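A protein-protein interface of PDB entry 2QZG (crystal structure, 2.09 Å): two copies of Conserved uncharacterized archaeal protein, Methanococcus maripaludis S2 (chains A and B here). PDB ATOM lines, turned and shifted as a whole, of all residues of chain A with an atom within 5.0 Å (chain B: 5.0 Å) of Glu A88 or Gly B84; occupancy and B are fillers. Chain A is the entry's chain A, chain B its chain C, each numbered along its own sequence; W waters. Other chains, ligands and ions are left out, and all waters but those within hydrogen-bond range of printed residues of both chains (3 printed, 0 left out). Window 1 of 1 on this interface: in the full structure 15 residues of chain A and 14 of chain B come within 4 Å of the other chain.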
ATOM      1  N   ILE A  19      21.279  19.123  -4.464  1.00  0.00           N
ATOM      2  CA  ILE A  19      21.926  18.142  -5.341  1.00  0.00           C
ATOM      3  C   ILE A  19      21.501  18.289  -6.828  1.00  0.00           C
ATOM      4  O   ILE A  19      22.345  18.221  -7.729  1.00  0.00           O
ATOM      5  CB  ILE A  19      21.691  16.705  -4.863  1.00  0.00           C
ATOM      6  CG1 ILE A  19      22.385  16.473  -3.500  1.00  0.00           C
ATOM      7  CG2 ILE A  19      22.215  15.716  -5.947  1.00  0.00           C
ATOM      8  CD1 ILE A  19      21.883  15.249  -2.699  1.00  0.00           C
ATOM      9  N   MET A  22      23.270  21.113  -8.364  1.00  0.00           N
ATOM     10  CA  MET A  22      24.672  20.787  -8.616  1.00  0.00           C
ATOM     11  C   MET A  22      24.761  19.982  -9.897  1.00  0.00           C
ATOM     12  O   MET A  22      25.656  20.204 -10.714  1.00  0.00           O
ATOM     13  CB  MET A  22      25.300  20.031  -7.448  1.00  0.00           C
ATOM     14  CG  MET A  22      25.868  20.908  -6.366  1.00  0.00           C
ATOM     15  SD  MET A  22      26.013  19.836  -4.752  1.00  0.00           S
ATOM     16  CE  MET A  22      27.916  19.417  -4.793  1.00  0.00           C
ATOM     17  N   TRP A  83      32.174  13.909  -7.301  1.00  0.00           N
ATOM     18  CA  TRP A  83      32.540  13.413  -5.980  1.00  0.00           C
ATOM     19  C   TRP A  83      31.730  14.062  -4.847  1.00  0.00           C
ATOM     20  O   TRP A  83      31.308  13.367  -3.903  1.00  0.00           O
ATOM     21  CB  TRP A  83      34.027  13.574  -5.733  1.00  0.00           C
ATOM     22  CG  TRP A  83      34.454  13.386  -4.315  1.00  0.00           C
ATOM     23  CD1 TRP A  83      34.328  12.264  -3.558  1.00  0.00           C
ATOM     24  CD2 TRP A  83      35.111  14.361  -3.489  1.00  0.00           C
ATOM     25  NE1 TRP A  83      34.874  12.481  -2.299  1.00  0.00           N
ATOM     26  CE2 TRP A  83      35.348  13.763  -2.237  1.00  0.00           C
ATOM     27  CE3 TRP A  83      35.520  15.679  -3.694  1.00  0.00           C
ATOM     28  CZ2 TRP A  83      35.977  14.439  -1.187  1.00  0.00           C
ATOM     29  CZ3 TRP A  83      36.149  16.357  -2.650  1.00  0.00           C
ATOM     30  CH2 TRP A  83      36.374  15.725  -1.417  1.00  0.00           C
ATOM     31  N   GLY A  84      31.539  15.385  -4.941  1.00  0.00           N
ATOM     32  CA  GLY A  84      30.747  16.149  -3.977  1.00  0.00           C
ATOM     33  C   GLY A  84      29.273  15.750  -4.002  1.00  0.00           C
ATOM     34  O   GLY A  84      28.660  15.540  -2.963  1.00  0.00           O
ATOM     35  N   ILE A  85      28.727  15.614  -5.204  1.00  0.00           N
ATOM     36  CA  ILE A  85      27.322  15.179  -5.403  1.00  0.00           C
ATOM     37  C   ILE A  85      27.085  13.770  -4.838  1.00  0.00           C
ATOM     38  O   ILE A  85      26.125  13.543  -4.104  1.00  0.00           O
ATOM     39  CB  ILE A  85      26.953  15.237  -6.898  1.00  0.00           C
ATOM     40  CG1 ILE A  85      26.907  16.698  -7.364  1.00  0.00           C
ATOM     41  CG2 ILE A  85      25.614  14.528  -7.169  1.00  0.00           C
ATOM     42  CD1 ILE A  85      26.808  16.880  -8.862  1.00  0.00           C
ATOM     43  N   VAL A  86      27.974  12.836  -5.181  1.00  0.00           N
ATOM     44  CA  VAL A  86      27.904  11.494  -4.664  1.00  0.00           C
ATOM     45  C   VAL A  86      28.037  11.439  -3.127  1.00  0.00           C
ATOM     46  O   VAL A  86      27.238  10.774  -2.462  1.00  0.00           O
ATOM     47  CB  VAL A  86      28.896  10.533  -5.362  1.00  0.00           C
ATOM     48  CG1 VAL A  86      29.004   9.164  -4.578  1.00  0.00           C
ATOM     49  CG2 VAL A  86      28.472  10.317  -6.843  1.00  0.00           C
ATOM     50  N   SER A  87      29.024  12.124  -2.566  1.00  0.00           N
ATOM     51  CA  SER A  87      29.174  12.168  -1.120  1.00  0.00           C
ATOM     52  C   SER A  87      27.890  12.695  -0.464  1.00  0.00           C
ATOM     53  O   SER A  87      27.477  12.179   0.575  1.00  0.00           O
ATOM     54  CB  SER A  87      30.368  13.047  -0.733  1.00  0.00           C
ATOM     55  OG  SER A  87      31.540  12.621  -1.407  1.00  0.00           O
ATOM     56  N   GLU A  88      27.265  13.719  -1.055  1.00  0.00           N
ATOM     57  CA  GLU A  88      26.024  14.242  -0.512  1.00  0.00           C
ATOM     58  C   GLU A  88      24.879  13.226  -0.597  1.00  0.00           C
ATOM     59  O   GLU A  88      24.139  13.062   0.350  1.00  0.00           O
ATOM     60  CB  GLU A  88      25.643  15.545  -1.201  1.00  0.00           C
ATOM     61  CG  GLU A  88      26.477  16.720  -0.686  1.00  0.00           C
ATOM     62  CD  GLU A  88      26.224  18.019  -1.434  1.00  0.00           C
ATOM     63  OE1 GLU A  88      25.471  18.010  -2.420  1.00  0.00           O
ATOM     64  OE2 GLU A  88      26.788  19.057  -1.024  1.00  0.00           O
ATOM     65  N   LEU A  89      24.749  12.570  -1.745  1.00  0.00           N
ATOM     66  CA  LEU A  89      23.788  11.491  -1.940  1.00  0.00           C
ATOM     67  C   LEU A  89      23.917  10.396  -0.876  1.00  0.00           C
ATOM     68  O   LEU A  89      22.908   9.885  -0.389  1.00  0.00           O
ATOM     69  CB  LEU A  89      23.900  10.907  -3.373  1.00  0.00           C
ATOM     70  CG  LEU A  89      23.322  11.804  -4.502  1.00  0.00           C
ATOM     71  CD1 LEU A  89      23.719  11.361  -5.886  1.00  0.00           C
ATOM     72  CD2 LEU A  89      21.814  11.905  -4.440  1.00  0.00           C
ATOM     73  N   GLU A  90      25.150  10.049  -0.516  1.00  0.00           N
ATOM     74  CA  GLU A  90      25.406   8.975   0.431  1.00  0.00           C
ATOM     75  C   GLU A  90      24.998   9.345   1.877  1.00  0.00           C
ATOM     76  O   GLU A  90      24.851   8.461   2.720  1.00  0.00           O
ATOM     77  CB  GLU A  90      26.879   8.517   0.351  1.00  0.00           C
ATOM     78  CG  GLU A  90      27.249   7.821  -0.988  1.00  0.00           C
ATOM     79  CD  GLU A  90      28.758   7.665  -1.224  1.00  0.00           C
ATOM     80  OE1 GLU A  90      29.569   8.461  -0.673  1.00  0.00           O
ATOM     81  OE2 GLU A  90      29.139   6.734  -1.977  1.00  0.00           O
ATOM     82  N   THR A  91      24.809  10.640   2.159  1.00  0.00           N
ATOM     83  CA  THR A  91      24.339  11.069   3.475  1.00  0.00           C
ATOM     84  C   THR A  91      22.829  10.916   3.637  1.00  0.00           C
ATOM     85  O   THR A  91      22.317  10.990   4.736  1.00  0.00           O
ATOM     86  CB  THR A  91      24.751  12.547   3.816  1.00  0.00           C
ATOM     87  OG1 THR A  91      24.034  13.470   2.976  1.00  0.00           O
ATOM     88  CG2 THR A  91      26.240  12.736   3.622  1.00  0.00           C
ATOM     89  N   ILE A  92      22.114  10.704   2.540  1.00  0.00           N
ATOM     90  CA  ILE A  92      20.659  10.661   2.584  1.00  0.00           C
ATOM     91  C   ILE A  92      20.150   9.351   3.201  1.00  0.00           C
ATOM     92  O   ILE A  92      20.382   8.275   2.653  1.00  0.00           O
ATOM     93  CB  ILE A  92      20.056  10.874   1.174  1.00  0.00           C
ATOM     94  CG1 ILE A  92      20.255  12.335   0.738  1.00  0.00           C
ATOM     95  CG2 ILE A  92      18.564  10.474   1.159  1.00  0.00           C
ATOM     96  CD1 ILE A  92      19.919  12.577  -0.697  1.00  0.00           C
ATOM     97  N   THR B  80      24.353  24.872   3.889  1.00  0.00           N
ATOM     98  CA  THR B  80      24.507  24.038   2.685  1.00  0.00           C
ATOM     99  C   THR B  80      25.964  23.738   2.372  1.00  0.00           C
ATOM    100  O   THR B  80      26.311  22.597   2.029  1.00  0.00           O
ATOM    101  CB  THR B  80      23.786  24.661   1.440  1.00  0.00           C
ATOM    102  OG1 THR B  80      22.372  24.547   1.615  1.00  0.00           O
ATOM    103  CG2 THR B  80      24.149  23.917   0.128  1.00  0.00           C
ATOM    104  N   GLN B  81      26.808  24.757   2.496  1.00  0.00           N
ATOM    105  CA  GLN B  81      28.238  24.588   2.277  1.00  0.00           C
ATOM    106  C   GLN B  81      28.791  23.591   3.275  1.00  0.00           C
ATOM    107  O   GLN B  81      29.552  22.715   2.897  1.00  0.00           O
ATOM    108  CB  GLN B  81      28.994  25.934   2.357  1.00  0.00           C
ATOM    109  CG  GLN B  81      28.734  26.835   1.144  1.00  0.00           C
ATOM    110  CD  GLN B  81      29.196  28.277   1.345  1.00  0.00           C
ATOM    111  OE1 GLN B  81      29.659  28.652   2.409  1.00  0.00           O
ATOM    112  NE2 GLN B  81      29.027  29.099   0.313  1.00  0.00           N
ATOM    113  N   ILE B  82      28.392  23.709   4.542  1.00  0.00           N
ATOM    114  CA  ILE B  82      28.887  22.804   5.578  1.00  0.00           C
ATOM    115  C   ILE B  82      28.403  21.356   5.385  1.00  0.00           C
ATOM    116  O   ILE B  82      29.177  20.434   5.588  1.00  0.00           O
ATOM    117  CB  ILE B  82      28.579  23.328   6.974  1.00  0.00           C
ATOM    118  CG1 ILE B  82      29.472  24.550   7.259  1.00  0.00           C
ATOM    119  CG2 ILE B  82      28.747  22.225   8.049  1.00  0.00           C
ATOM    120  CD1 ILE B  82      28.957  25.421   8.319  1.00  0.00           C
ATOM    121  N   TRP B  83      27.144  21.177   4.979  1.00  0.00           N
ATOM    122  CA  TRP B  83      26.607  19.858   4.632  1.00  0.00           C
ATOM    123  C   TRP B  83      27.467  19.182   3.542  1.00  0.00           C
ATOM    124  O   TRP B  83      27.874  18.035   3.694  1.00  0.00           O
ATOM    125  CB  TRP B  83      25.126  19.935   4.241  1.00  0.00           C
ATOM    126  CG  TRP B  83      24.589  18.644   3.626  1.00  0.00           C
ATOM    127  CD1 TRP B  83      24.627  17.395   4.180  1.00  0.00           C
ATOM    128  CD2 TRP B  83      23.953  18.497   2.355  1.00  0.00           C
ATOM    129  NE1 TRP B  83      24.043  16.477   3.329  1.00  0.00           N
ATOM    130  CE2 TRP B  83      23.616  17.134   2.206  1.00  0.00           C
ATOM    131  CE3 TRP B  83      23.615  19.391   1.331  1.00  0.00           C
ATOM    132  CZ2 TRP B  83      22.975  16.639   1.067  1.00  0.00           C
ATOM    133  CZ3 TRP B  83      22.958  18.896   0.203  1.00  0.00           C
ATOM    134  CH2 TRP B  83      22.641  17.540   0.088  1.00  0.00           C
ATOM    135  N   GLY B  84      27.833  19.940   2.506  1.00  0.00           N
ATOM    136  CA  GLY B  84      28.732  19.442   1.479  1.00  0.00           C
ATOM    137  C   GLY B  84      30.134  19.071   1.948  1.00  0.00           C
ATOM    138  O   GLY B  84      30.644  18.036   1.534  1.00  0.00           O
ATOM    139  N   ILE B  85      30.760  19.919   2.777  1.00  0.00           N
ATOM    140  CA  ILE B  85      32.061  19.650   3.376  1.00  0.00           C
ATOM    141  C   ILE B  85      31.999  18.430   4.316  1.00  0.00           C
ATOM    142  O   ILE B  85      32.875  17.572   4.269  1.00  0.00           O
ATOM    143  CB  ILE B  85      32.594  20.887   4.174  1.00  0.00           C
ATOM    144  CG1 ILE B  85      32.818  22.092   3.250  1.00  0.00           C
ATOM    145  CG2 ILE B  85      33.857  20.522   4.960  1.00  0.00           C
ATOM    146  CD1 ILE B  85      32.846  23.458   3.987  1.00  0.00           C
ATOM    147  N   VAL B  86      30.973  18.345   5.166  1.00  0.00           N
ATOM    148  CA  VAL B  86      30.841  17.182   6.074  1.00  0.00           C
ATOM    149  C   VAL B  86      30.678  15.891   5.274  1.00  0.00           C
ATOM    150  O   VAL B  86      31.351  14.894   5.554  1.00  0.00           O
ATOM    151  CB  VAL B  86      29.683  17.366   7.087  1.00  0.00           C
ATOM    152  CG1 VAL B  86      29.328  16.029   7.819  1.00  0.00           C
ATOM    153  CG2 VAL B  86      30.058  18.461   8.101  1.00  0.00           C
ATOM    154  N   SER B  87      29.797  15.925   4.269  1.00  0.00           N
ATOM    155  CA  SER B  87      29.564  14.779   3.380  1.00  0.00           C
ATOM    156  C   SER B  87      30.869  14.269   2.774  1.00  0.00           C
ATOM    157  O   SER B  87      31.120  13.080   2.730  1.00  0.00           O
ATOM    158  CB  SER B  87      28.616  15.184   2.259  1.00  0.00           C
ATOM    159  OG  SER B  87      27.389  15.575   2.824  1.00  0.00           O
ATOM    160  N   GLU B  88      31.664  15.195   2.267  1.00  0.00           N
ATOM    161  CA  GLU B  88      32.957  14.864   1.686  1.00  0.00           C
ATOM    162  C   GLU B  88      33.956  14.357   2.721  1.00  0.00           C
ATOM    163  O   GLU B  88      34.638  13.364   2.462  1.00  0.00           O
ATOM    164  CB  GLU B  88      33.513  16.056   0.945  1.00  0.00           C
ATOM    165  CG  GLU B  88      32.708  16.445  -0.292  1.00  0.00           C
ATOM    166  CD  GLU B  88      33.174  17.782  -0.843  1.00  0.00           C
ATOM    167  OE1 GLU B  88      34.224  18.243  -0.387  1.00  0.00           O
ATOM    168  OE2 GLU B  88      32.516  18.370  -1.725  1.00  0.00           O
HETATM  169  O   HOH W   1      29.882  19.021  -1.801  1.00  0.00           O
HETATM  170  O   HOH W   2      26.543  21.687  -0.894  1.00  0.00           O
HETATM  171  O   HOH W   3      29.212  11.210   2.388  1.00  0.00           O
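OG1 of Thr A91 lies within hydrogen-bond range of NE1 of Trp B83, 3.0 Å away.
O of Trp A83 is in hydrogen-bond range of OG of Ser A87 (2.6 Å).
The side-chain hydroxyl of Thr A91 is in hydrogen-bond range of the backbone carbonyl oxygen of Glu A88, at 2.7 Å.
The backbone carbonyl oxygen (O) of Trp B83 is in hydrogen-bond range of the side-chain hydroxyl (OG) of Ser B87, at 2.7 Å.
Among the printed residues, pairs that only touch across the chains: Thr A91 with Ser B87, Glu A88 with Gly B84, Trp A83 with Glu B88, Ser A87 with Ser B87, Gly A84 with Glu B88, Glu A88 with Trp B83, Ile A19 with Trp B83, Glu A88 with Ser B87 and Ser A87 with Glu B88.
Of the printed residues of chain B, Gly A84 touches Glu B88.
Of the printed residues of chain B, Ser A87 touches Ser B87 (3.5 Å) and Glu B88 (3.9 Å).
Glu A88 touches just these residues of chain B: Trp B83, Gly B84 and Ser B87.
Of the printed residues of chain B, Thr A91 touches Trp B83 and Ser B87.
Of the printed residues of chain A, Trp B83 touches Ile A19, Glu A88 and Thr A91.
Of chain A, only Glu A88 comes within 4 Å of Gly B84.
Of the printed residues of chain A, Glu B88 touches Trp A83, Gly A84 and Ser A87.
The nearest printed residue of chain A that does not touch Gly B84 is Ser A87 (5.5 Å).
The nearest printed residue of chain B that does not touch Thr A91 is Val B86 (5.7 Å).
Printed residues of chain A that touch a printed residue of chain B: Ile A19, Trp A83, Gly A84, Ser A87, Glu A88 and Thr A91.
Among the printed residues, no Asp or Glu carboxylate lies within 4 Å of a Lys or Arg side-chain nitrogen of the other chain.
Trp A83 touches Glu B88, and with the chains exchanged Glu A88 touches Trp B83.
Gly A84 touches Glu B88, and with the chains exchanged Glu A88 touches Gly B84.
Ser B87 touches its own counterpart, Ser A87.
Ser A87 touches Glu B88, and with the chains exchanged Glu A88 touches Ser B87.
Positions printed for both chains: 83, 84, 85, 86, 87 and 88.
Of the 10 pairs that touch across the chains among the printed residues, 7 have their exchanged pair printed and touching as well.
Water W2 lies within hydrogen-bond range of the side-chain carboxylate of Glu A88 (2.6 Å) and the backbone carbonyl oxygen of Thr B80 (3.1 Å).
Water W3 bridges O of Ser A87 and O of Ser B87.
Water W1 bridges OE2 of Glu B88 and OE2 of Glu A88.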
